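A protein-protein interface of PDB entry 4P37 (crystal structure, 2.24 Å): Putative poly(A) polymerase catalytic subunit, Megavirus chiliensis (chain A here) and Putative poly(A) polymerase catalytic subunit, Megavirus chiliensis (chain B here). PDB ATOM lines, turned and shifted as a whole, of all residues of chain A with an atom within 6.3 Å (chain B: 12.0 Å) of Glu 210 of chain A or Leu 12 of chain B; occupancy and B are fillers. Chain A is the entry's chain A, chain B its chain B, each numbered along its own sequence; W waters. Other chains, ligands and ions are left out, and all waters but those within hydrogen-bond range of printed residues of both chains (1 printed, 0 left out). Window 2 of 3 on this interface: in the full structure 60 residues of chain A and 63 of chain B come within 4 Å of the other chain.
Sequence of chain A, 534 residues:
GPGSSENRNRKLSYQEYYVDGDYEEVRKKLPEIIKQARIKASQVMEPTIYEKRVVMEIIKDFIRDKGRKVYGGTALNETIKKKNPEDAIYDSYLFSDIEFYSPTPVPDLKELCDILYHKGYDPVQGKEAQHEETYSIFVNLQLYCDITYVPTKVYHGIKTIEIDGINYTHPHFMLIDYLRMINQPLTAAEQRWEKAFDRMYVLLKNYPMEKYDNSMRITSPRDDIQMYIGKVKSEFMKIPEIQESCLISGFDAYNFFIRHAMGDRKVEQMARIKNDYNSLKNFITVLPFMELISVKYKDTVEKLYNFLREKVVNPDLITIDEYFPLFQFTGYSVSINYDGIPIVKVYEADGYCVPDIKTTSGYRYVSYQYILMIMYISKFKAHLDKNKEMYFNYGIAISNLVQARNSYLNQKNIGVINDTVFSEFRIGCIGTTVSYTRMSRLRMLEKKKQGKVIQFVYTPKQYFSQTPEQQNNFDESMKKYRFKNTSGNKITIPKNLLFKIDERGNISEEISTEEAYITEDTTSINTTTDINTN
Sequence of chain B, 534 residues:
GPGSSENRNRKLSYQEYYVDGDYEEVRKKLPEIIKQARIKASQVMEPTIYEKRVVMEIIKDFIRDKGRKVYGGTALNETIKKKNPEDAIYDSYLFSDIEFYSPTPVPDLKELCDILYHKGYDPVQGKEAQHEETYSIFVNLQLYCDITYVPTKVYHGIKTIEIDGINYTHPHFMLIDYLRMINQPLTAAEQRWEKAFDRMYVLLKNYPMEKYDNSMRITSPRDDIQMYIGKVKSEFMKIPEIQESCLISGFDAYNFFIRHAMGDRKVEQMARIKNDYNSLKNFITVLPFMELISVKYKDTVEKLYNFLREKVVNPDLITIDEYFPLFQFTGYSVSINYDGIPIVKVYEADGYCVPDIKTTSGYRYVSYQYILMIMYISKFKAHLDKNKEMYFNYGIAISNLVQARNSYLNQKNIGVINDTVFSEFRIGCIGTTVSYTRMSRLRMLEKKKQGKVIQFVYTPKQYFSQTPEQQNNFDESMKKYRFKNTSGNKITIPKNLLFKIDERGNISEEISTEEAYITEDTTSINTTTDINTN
The backbone carbonyl oxygen (O) of Met 209 of chain A lies within hydrogen-bond range of the backbone NH (N) of Gln 15 of chain B (2.8 Å). The backbone carbonyl oxygen (O) of Glu 210 of chain A lies within hydrogen-bond range of the side-chain amide nitrogen (NE2) of Gln 15 of chain B (3.1 Å). The backbone NH of Lys 211 of chain A lies within hydrogen-bond range of the backbone carbonyl oxygen of Ser 13 of chain B, at 3.0 Å. The backbone carbonyl oxygen (O) of Ser 399 of chain A lies within hydrogen-bond range of the side-chain amide nitrogen (NE2) of Gln 15 of chain B (3.0 Å).
The side-chain hydroxyl (OH) of Tyr 212 of chain A is in hydrogen-bond range of the side-chain carboxylate (OE1) of Glu 210 of chain A. The side-chain hydroxyl of Ser 399 of chain A is in hydrogen-bond range of the backbone NH of Tyr 212 of chain A, 2.8 Å away.
Pro 208 of chain A touches Tyr 14 of chain B (CG to CD2, 3.6 Å). Pro 208 of chain A touches Gln 15 of chain B (CB to O, 3.8 Å). Tyr 14 of chain B touches Met 209 of chain A. Tyr 17 of chain B touches Met 209 of chain A. CD2 of Leu 12 of chain B touches OE1 of Glu 210 of chain A, at 3.4 Å. Glu 210 of chain A touches Ser 13 of chain B (CA to O, 3.7 Å). Tyr 14 of chain B touches Lys 211 of chain A. Gln 15 of chain B touches Lys 211 of chain A (NE2 to CD, 3.7 Å). CG1 of Val 402 of chain A touches OE1 of Gln 15 of chain B (3.7 Å). Tyr 17 of chain B touches Val 402 of chain A.
Of the printed residues of chain B, Pro 208 of chain A touches Tyr 14 (3.6 Å) and Gln 15 (3.8 Å). Of chain B, only Tyr 14, Gln 15 and Tyr 17 come within 4 Å of Met 209 of chain A. Glu 210 of chain A touches three residues of chain B. Lys 211 of chain A touches just these residues of chain B: Ser 13 (3.0 Å), Tyr 14 (3.97 Å) and Gln 15 (3.7 Å). Tyr 212 of chain A touches none of the printed residues of chain B. Gly 395 of chain A touches none of the printed residues of chain B. Ile 398 of chain A touches none of the printed residues of chain B. Ser 399 of chain A touches one residue of chain B. Printed residues of chain B within 4 Å of Val 402 of chain A: Gln 15 and Tyr 17. Leu 12 of chain B touches one residue of chain A. Printed residues of chain A within 4 Å of Tyr 14 of chain B: Pro 208 (3.6 Å), Met 209 (3.4 Å) and Lys 211 (3.97 Å). The nearest residue of chain A that does not touch Leu 12 of chain B is Tyr 212 of chain A (5.4 Å). The nearest printed residue of chain B that does not touch Val 402 of chain A is Glu 16 of chain B (5.5 Å).
Of the 12 printed residues of chain B, 5 touch a printed residue of chain A. Hydrophobic or aromatic side chains of chain B within 4 Å of the printed part of chain A: Leu 12, Tyr 14 and Tyr 17. Hydrophobic or aromatic side chains of chain A within 4 Å of the printed part of chain B: Pro 208, Met 209 and Val 402. Among the printed residues, 14 pairs touch across the chains.
Water W1 lies within hydrogen-bond range of the backbone carbonyl oxygen of Gln 15 of chain B (2.8 Å), the backbone NH of Met 209 of chain A (2.8 Å) and the backbone NH of Tyr 17 of chain B (3.4 Å).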
ATOM      1  N   HIS A 172      15.628  -9.798 -22.275  1.00  0.00           N
ATOM      2  CA  HIS A 172      17.019 -10.246 -22.222  1.00  0.00           C
ATOM      3  C   HIS A 172      17.356 -10.969 -20.908  1.00  0.00           C
ATOM      4  O   HIS A 172      18.413 -11.599 -20.822  1.00  0.00           O
ATOM      5  CB  HIS A 172      18.013  -9.142 -22.593  1.00  0.00           C
ATOM      6  CG  HIS A 172      18.132  -9.021 -24.084  1.00  0.00           C
ATOM      7  ND1 HIS A 172      18.947  -9.885 -24.822  1.00  0.00           N
ATOM      8  CD2 HIS A 172      17.423  -8.257 -24.948  1.00  0.00           C
ATOM      9  CE1 HIS A 172      18.744  -9.581 -26.095  1.00  0.00           C
ATOM     10  NE2 HIS A 172      17.842  -8.606 -26.225  1.00  0.00           N
ATOM     11  N   PRO A 208      16.716  -6.631 -30.163  1.00  0.00           N
ATOM     12  CA  PRO A 208      18.000  -7.165 -30.649  1.00  0.00           C
ATOM     13  C   PRO A 208      19.171  -7.065 -29.693  1.00  0.00           C
ATOM     14  O   PRO A 208      19.124  -6.332 -28.712  1.00  0.00           O
ATOM     15  CB  PRO A 208      18.252  -6.368 -31.945  1.00  0.00           C
ATOM     16  CG  PRO A 208      17.466  -5.145 -31.811  1.00  0.00           C
ATOM     17  CD  PRO A 208      16.294  -5.441 -30.946  1.00  0.00           C
ATOM     18  N   MET A 209      20.245  -7.812 -30.017  1.00  0.00           N
ATOM     19  CA  MET A 209      21.541  -7.781 -29.321  1.00  0.00           C
ATOM     20  C   MET A 209      22.100  -6.367 -29.483  1.00  0.00           C
ATOM     21  O   MET A 209      22.041  -5.803 -30.576  1.00  0.00           O
ATOM     22  CB  MET A 209      22.520  -8.742 -30.010  1.00  0.00           C
ATOM     23  CG  MET A 209      22.129 -10.198 -29.885  1.00  0.00           C
ATOM     24  SD  MET A 209      22.090 -10.752 -27.991  1.00  0.00           S
ATOM     25  CE  MET A 209      22.075 -12.708 -28.418  1.00  0.00           C
ATOM     26  N   GLU A 210      22.582  -5.772 -28.409  1.00  0.00           N
ATOM     27  CA  GLU A 210      23.115  -4.418 -28.494  1.00  0.00           C
ATOM     28  C   GLU A 210      24.522  -4.420 -29.094  1.00  0.00           C
ATOM     29  O   GLU A 210      25.214  -5.448 -29.106  1.00  0.00           O
ATOM     30  CB  GLU A 210      23.136  -3.766 -27.110  1.00  0.00           C
ATOM     31  CG  GLU A 210      21.766  -3.332 -26.615  1.00  0.00           C
ATOM     32  CD  GLU A 210      21.808  -2.419 -25.408  1.00  0.00           C
ATOM     33  OE1 GLU A 210      22.522  -1.391 -25.459  1.00  0.00           O
ATOM     34  OE2 GLU A 210      21.150  -2.750 -24.396  1.00  0.00           O
ATOM     35  N   LYS A 211      24.934  -3.267 -29.595  1.00  0.00           N
ATOM     36  CA  LYS A 211      26.284  -3.108 -30.105  1.00  0.00           C
ATOM     37  C   LYS A 211      27.010  -2.124 -29.197  1.00  0.00           C
ATOM     38  O   LYS A 211      26.527  -1.007 -28.991  1.00  0.00           O
ATOM     39  CB  LYS A 211      26.289  -2.648 -31.575  1.00  0.00           C
ATOM     40  CG  LYS A 211      27.682  -2.317 -32.115  1.00  0.00           C
ATOM     41  CD  LYS A 211      28.521  -3.572 -32.397  1.00  0.00           C
ATOM     42  CE  LYS A 211      29.917  -3.218 -32.842  1.00  0.00           C
ATOM     43  NZ  LYS A 211      30.760  -2.746 -31.711  1.00  0.00           N
ATOM     44  N   TYR A 212      28.146  -2.553 -28.631  1.00  0.00           N
ATOM     45  CA  TYR A 212      28.967  -1.711 -27.766  1.00  0.00           C
ATOM     46  C   TYR A 212      30.299  -1.428 -28.419  1.00  0.00           C
ATOM     47  O   TYR A 212      30.945  -2.333 -28.956  1.00  0.00           O
ATOM     48  CB  TYR A 212      29.132  -2.299 -26.357  1.00  0.00           C
ATOM     49  CG  TYR A 212      27.821  -2.457 -25.621  1.00  0.00           C
ATOM     50  CD1 TYR A 212      26.933  -1.394 -25.500  1.00  0.00           C
ATOM     51  CD2 TYR A 212      27.476  -3.666 -25.029  1.00  0.00           C
ATOM     52  CE1 TYR A 212      25.726  -1.538 -24.827  1.00  0.00           C
ATOM     53  CE2 TYR A 212      26.273  -3.823 -24.354  1.00  0.00           C
ATOM     54  CZ  TYR A 212      25.396  -2.760 -24.258  1.00  0.00           C
ATOM     55  OH  TYR A 212      24.222  -2.932 -23.568  1.00  0.00           O
ATOM     56  N   GLY A 395      29.033  -7.068 -20.442  1.00  0.00           N
ATOM     57  CA  GLY A 395      28.198  -6.454 -21.485  1.00  0.00           C
ATOM     58  C   GLY A 395      28.952  -6.300 -22.796  1.00  0.00           C
ATOM     59  O   GLY A 395      28.434  -6.654 -23.864  1.00  0.00           O
ATOM     60  N   ILE A 398      29.633  -9.776 -24.387  1.00  0.00           N
ATOM     61  CA  ILE A 398      28.434 -10.244 -25.102  1.00  0.00           C
ATOM     62  C   ILE A 398      28.424  -9.627 -26.512  1.00  0.00           C
ATOM     63  O   ILE A 398      28.331 -10.359 -27.505  1.00  0.00           O
ATOM     64  CB  ILE A 398      27.089  -9.979 -24.336  1.00  0.00           C
ATOM     65  CG1 ILE A 398      27.012 -10.804 -23.011  1.00  0.00           C
ATOM     66  CG2 ILE A 398      25.890 -10.316 -25.238  1.00  0.00           C
ATOM     67  CD1 ILE A 398      25.932 -10.346 -21.980  1.00  0.00           C
ATOM     68  N   SER A 399      28.552  -8.285 -26.588  1.00  0.00           N
ATOM     69  CA  SER A 399      28.584  -7.520 -27.845  1.00  0.00           C
ATOM     70  C   SER A 399      29.688  -8.065 -28.771  1.00  0.00           C
ATOM     71  O   SER A 399      29.391  -8.433 -29.909  1.00  0.00           O
ATOM     72  CB  SER A 399      28.756  -6.028 -27.564  1.00  0.00           C
ATOM     73  OG  SER A 399      28.808  -5.282 -28.767  1.00  0.00           O
ATOM     74  N   VAL A 402      28.835 -11.724 -30.144  1.00  0.00           N
ATOM     75  CA  VAL A 402      27.816 -11.683 -31.194  1.00  0.00           C
ATOM     76  C   VAL A 402      28.500 -11.196 -32.489  1.00  0.00           C
ATOM     77  O   VAL A 402      28.347 -11.842 -33.533  1.00  0.00           O
ATOM     78  CB  VAL A 402      26.611 -10.810 -30.768  1.00  0.00           C
ATOM     79  CG1 VAL A 402      25.645 -10.572 -31.934  1.00  0.00           C
ATOM     80  CG2 VAL A 402      25.879 -11.454 -29.585  1.00  0.00           C
ATOM     81  N   ASN B   7      13.095  11.888 -29.634  1.00  0.00           N
ATOM     82  CA  ASN B   7      13.787  12.312 -28.418  1.00  0.00           C
ATOM     83  C   ASN B   7      13.809  11.199 -27.320  1.00  0.00           C
ATOM     84  O   ASN B   7      13.955  11.509 -26.129  1.00  0.00           O
ATOM     85  CB  ASN B   7      13.174  13.628 -27.892  1.00  0.00           C
ATOM     86  CG  ASN B   7      13.529  14.890 -28.660  1.00  0.00           C
ATOM     87  OD1 ASN B   7      14.015  15.873 -28.084  1.00  0.00           O
ATOM     88  ND2 ASN B   7      13.218  14.938 -29.956  1.00  0.00           N
ATOM     89  N   ARG B   8      13.682   9.906 -27.732  1.00  0.00           N
ATOM     90  CA  ARG B   8      13.707   8.743 -26.832  1.00  0.00           C
ATOM     91  C   ARG B   8      15.156   8.540 -26.326  1.00  0.00           C
ATOM     92  O   ARG B   8      15.502   9.074 -25.268  1.00  0.00           O
ATOM     93  CB  ARG B   8      13.133   7.495 -27.540  1.00  0.00           C
ATOM     94  CG  ARG B   8      12.174   6.694 -26.662  1.00  0.00           C
ATOM     95  CD  ARG B   8      11.474   5.578 -27.423  1.00  0.00           C
ATOM     96  NE  ARG B   8      12.291   4.366 -27.523  1.00  0.00           N
ATOM     97  CZ  ARG B   8      11.904   3.240 -28.120  1.00  0.00           C
ATOM     98  NH1 ARG B   8      12.715   2.190 -28.158  1.00  0.00           N
ATOM     99  NH2 ARG B   8      10.704   3.156 -28.684  1.00  0.00           N
ATOM    100  N   ASN B   9      15.999   7.807 -27.101  1.00  0.00           N
ATOM    101  CA  ASN B   9      17.441   7.590 -26.893  1.00  0.00           C
ATOM    102  C   ASN B   9      18.090   7.243 -28.235  1.00  0.00           C
ATOM    103  O   ASN B   9      17.930   6.139 -28.771  1.00  0.00           O
ATOM    104  CB  ASN B   9      17.782   6.580 -25.797  1.00  0.00           C
ATOM    105  CG  ASN B   9      19.271   6.505 -25.506  1.00  0.00           C
ATOM    106  OD1 ASN B   9      19.993   7.508 -25.512  1.00  0.00           O
ATOM    107  ND2 ASN B   9      19.770   5.309 -25.256  1.00  0.00           N
ATOM    108  N   ARG B  10      18.798   8.228 -28.780  1.00  0.00           N
ATOM    109  CA  ARG B  10      19.413   8.186 -30.104  1.00  0.00           C
ATOM    110  C   ARG B  10      20.709   7.382 -30.194  1.00  0.00           C
ATOM    111  O   ARG B  10      20.970   6.793 -31.244  1.00  0.00           O
ATOM    112  CB  ARG B  10      19.634   9.614 -30.631  1.00  0.00           C
ATOM    113  CG  ARG B  10      18.399  10.503 -30.560  1.00  0.00           C
ATOM    114  CD  ARG B  10      18.651  11.834 -31.233  1.00  0.00           C
ATOM    115  NE  ARG B  10      17.470  12.698 -31.196  1.00  0.00           N
ATOM    116  CZ  ARG B  10      16.505  12.692 -32.111  1.00  0.00           C
ATOM    117  NH1 ARG B  10      16.572  11.868 -33.155  1.00  0.00           N
ATOM    118  NH2 ARG B  10      15.467  13.509 -31.993  1.00  0.00           N
ATOM    119  N   LYS B  11      21.513   7.372 -29.107  1.00  0.00           N
ATOM    120  CA  LYS B  11      22.824   6.712 -29.028  1.00  0.00           C
ATOM    121  C   LYS B  11      22.840   5.165 -29.194  1.00  0.00           C
ATOM    122  O   LYS B  11      23.933   4.602 -29.315  1.00  0.00           O
ATOM    123  CB  LYS B  11      23.530   7.080 -27.713  1.00  0.00           C
ATOM    124  CG  LYS B  11      23.874   8.551 -27.538  1.00  0.00           C
ATOM    125  CD  LYS B  11      24.390   8.796 -26.124  1.00  0.00           C
ATOM    126  CE  LYS B  11      25.248  10.028 -26.010  1.00  0.00           C
ATOM    127  NZ  LYS B  11      24.438  11.275 -26.035  1.00  0.00           N
ATOM    128  N   LEU B  12      21.678   4.474 -29.216  1.00  0.00           N
ATOM    129  CA  LEU B  12      21.716   3.006 -29.277  1.00  0.00           C
ATOM    130  C   LEU B  12      21.868   2.370 -30.684  1.00  0.00           C
ATOM    131  O   LEU B  12      21.121   2.645 -31.627  1.00  0.00           O
ATOM    132  CB  LEU B  12      20.533   2.359 -28.536  1.00  0.00           C
ATOM    133  CG  LEU B  12      20.553   2.534 -26.990  1.00  0.00           C
ATOM    134  CD1 LEU B  12      19.269   2.045 -26.362  1.00  0.00           C
ATOM    135  CD2 LEU B  12      21.760   1.829 -26.328  1.00  0.00           C
ATOM    136  N   SER B  13      22.866   1.479 -30.765  1.00  0.00           N
ATOM    137  CA  SER B  13      23.229   0.655 -31.902  1.00  0.00           C
ATOM    138  C   SER B  13      22.896  -0.798 -31.559  1.00  0.00           C
ATOM    139  O   SER B  13      22.960  -1.202 -30.390  1.00  0.00           O
ATOM    140  CB  SER B  13      24.711   0.820 -32.229  1.00  0.00           C
ATOM    141  OG  SER B  13      25.011   2.170 -32.550  1.00  0.00           O
ATOM    142  N   TYR B  14      22.504  -1.572 -32.570  1.00  0.00           N
ATOM    143  CA  TYR B  14      22.127  -2.964 -32.379  1.00  0.00           C
ATOM    144  C   TYR B  14      22.771  -3.857 -33.421  1.00  0.00           C
ATOM    145  O   TYR B  14      23.284  -3.349 -34.416  1.00  0.00           O
ATOM    146  CB  TYR B  14      20.587  -3.114 -32.348  1.00  0.00           C
ATOM    147  CG  TYR B  14      19.876  -2.848 -33.661  1.00  0.00           C
ATOM    148  CD1 TYR B  14      19.526  -1.551 -34.041  1.00  0.00           C
ATOM    149  CD2 TYR B  14      19.483  -3.898 -34.491  1.00  0.00           C
ATOM    150  CE1 TYR B  14      18.875  -1.301 -35.253  1.00  0.00           C
ATOM    151  CE2 TYR B  14      18.816  -3.662 -35.693  1.00  0.00           C
ATOM    152  CZ  TYR B  14      18.516  -2.361 -36.069  1.00  0.00           C
ATOM    153  OH  TYR B  14      17.862  -2.114 -37.248  1.00  0.00           O
ATOM    154  N   GLN B  15      22.784  -5.179 -33.182  1.00  0.00           N
ATOM    155  CA  GLN B  15      23.346  -6.151 -34.139  1.00  0.00           C
ATOM    156  C   GLN B  15      22.256  -7.080 -34.571  1.00  0.00           C
ATOM    157  O   GLN B  15      21.394  -7.390 -33.765  1.00  0.00           O
ATOM    158  CB  GLN B  15      24.486  -7.006 -33.534  1.00  0.00           C
ATOM    159  CG  GLN B  15      25.458  -6.212 -32.705  1.00  0.00           C
ATOM    160  CD  GLN B  15      26.721  -6.949 -32.367  1.00  0.00           C
ATOM    161  OE1 GLN B  15      27.357  -7.600 -33.203  1.00  0.00           O
ATOM    162  NE2 GLN B  15      27.177  -6.766 -31.146  1.00  0.00           N
ATOM    163  N   GLU B  16      22.296  -7.587 -35.807  1.00  0.00           N
ATOM    164  CA  GLU B  16      21.300  -8.559 -36.262  1.00  0.00           C
ATOM    165  C   GLU B  16      21.852  -9.997 -36.046  1.00  0.00           C
ATOM    166  O   GLU B  16      22.822 -10.392 -36.689  1.00  0.00           O
ATOM    167  CB  GLU B  16      20.907  -8.289 -37.723  1.00  0.00           C
ATOM    168  CG  GLU B  16      19.506  -8.762 -38.067  1.00  0.00           C
ATOM    169  CD  GLU B  16      18.894  -8.274 -39.370  1.00  0.00           C
ATOM    170  OE1 GLU B  16      19.652  -7.970 -40.322  1.00  0.00           O
ATOM    171  OE2 GLU B  16      17.641  -8.262 -39.457  1.00  0.00           O
ATOM    172  N   TYR B  17      21.261 -10.747 -35.101  1.00  0.00           N
ATOM    173  CA  TYR B  17      21.637 -12.101 -34.698  1.00  0.00           C
ATOM    174  C   TYR B  17      21.077 -13.103 -35.690  1.00  0.00           C
ATOM    175  O   TYR B  17      21.817 -13.968 -36.142  1.00  0.00           O
ATOM    176  CB  TYR B  17      21.207 -12.360 -33.226  1.00  0.00           C
ATOM    177  CG  TYR B  17      21.840 -13.607 -32.667  1.00  0.00           C
ATOM    178  CD1 TYR B  17      23.130 -13.586 -32.153  1.00  0.00           C
ATOM    179  CD2 TYR B  17      21.179 -14.830 -32.727  1.00  0.00           C
ATOM    180  CE1 TYR B  17      23.731 -14.744 -31.662  1.00  0.00           C
ATOM    181  CE2 TYR B  17      21.784 -15.999 -32.283  1.00  0.00           C
ATOM    182  CZ  TYR B  17      23.061 -15.953 -31.749  1.00  0.00           C
ATOM    183  OH  TYR B  17      23.643 -17.115 -31.290  1.00  0.00           O
ATOM    184  N   TYR B  18      19.793 -12.988 -36.035  1.00  0.00           N
ATOM    185  CA  TYR B  18      19.160 -13.806 -37.066  1.00  0.00           C
ATOM    186  C   TYR B  18      18.655 -12.875 -38.177  1.00  0.00           C
ATOM    187  O   TYR B  18      18.057 -11.840 -37.896  1.00  0.00           O
ATOM    188  CB  TYR B  18      17.997 -14.676 -36.545  1.00  0.00           C
ATOM    189  CG  TYR B  18      18.373 -15.728 -35.533  1.00  0.00           C
ATOM    190  CD1 TYR B  18      19.260 -16.751 -35.854  1.00  0.00           C
ATOM    191  CD2 TYR B  18      17.790 -15.742 -34.270  1.00  0.00           C
ATOM    192  CE1 TYR B  18      19.600 -17.733 -34.921  1.00  0.00           C
ATOM    193  CE2 TYR B  18      18.125 -16.711 -33.328  1.00  0.00           C
ATOM    194  CZ  TYR B  18      19.033 -17.701 -33.657  1.00  0.00           C
ATOM    195  OH  TYR B  18      19.318 -18.661 -32.732  1.00  0.00           O
HETATM  196  O   HOH W   1      19.905  -9.295 -32.396  1.00  0.00           O
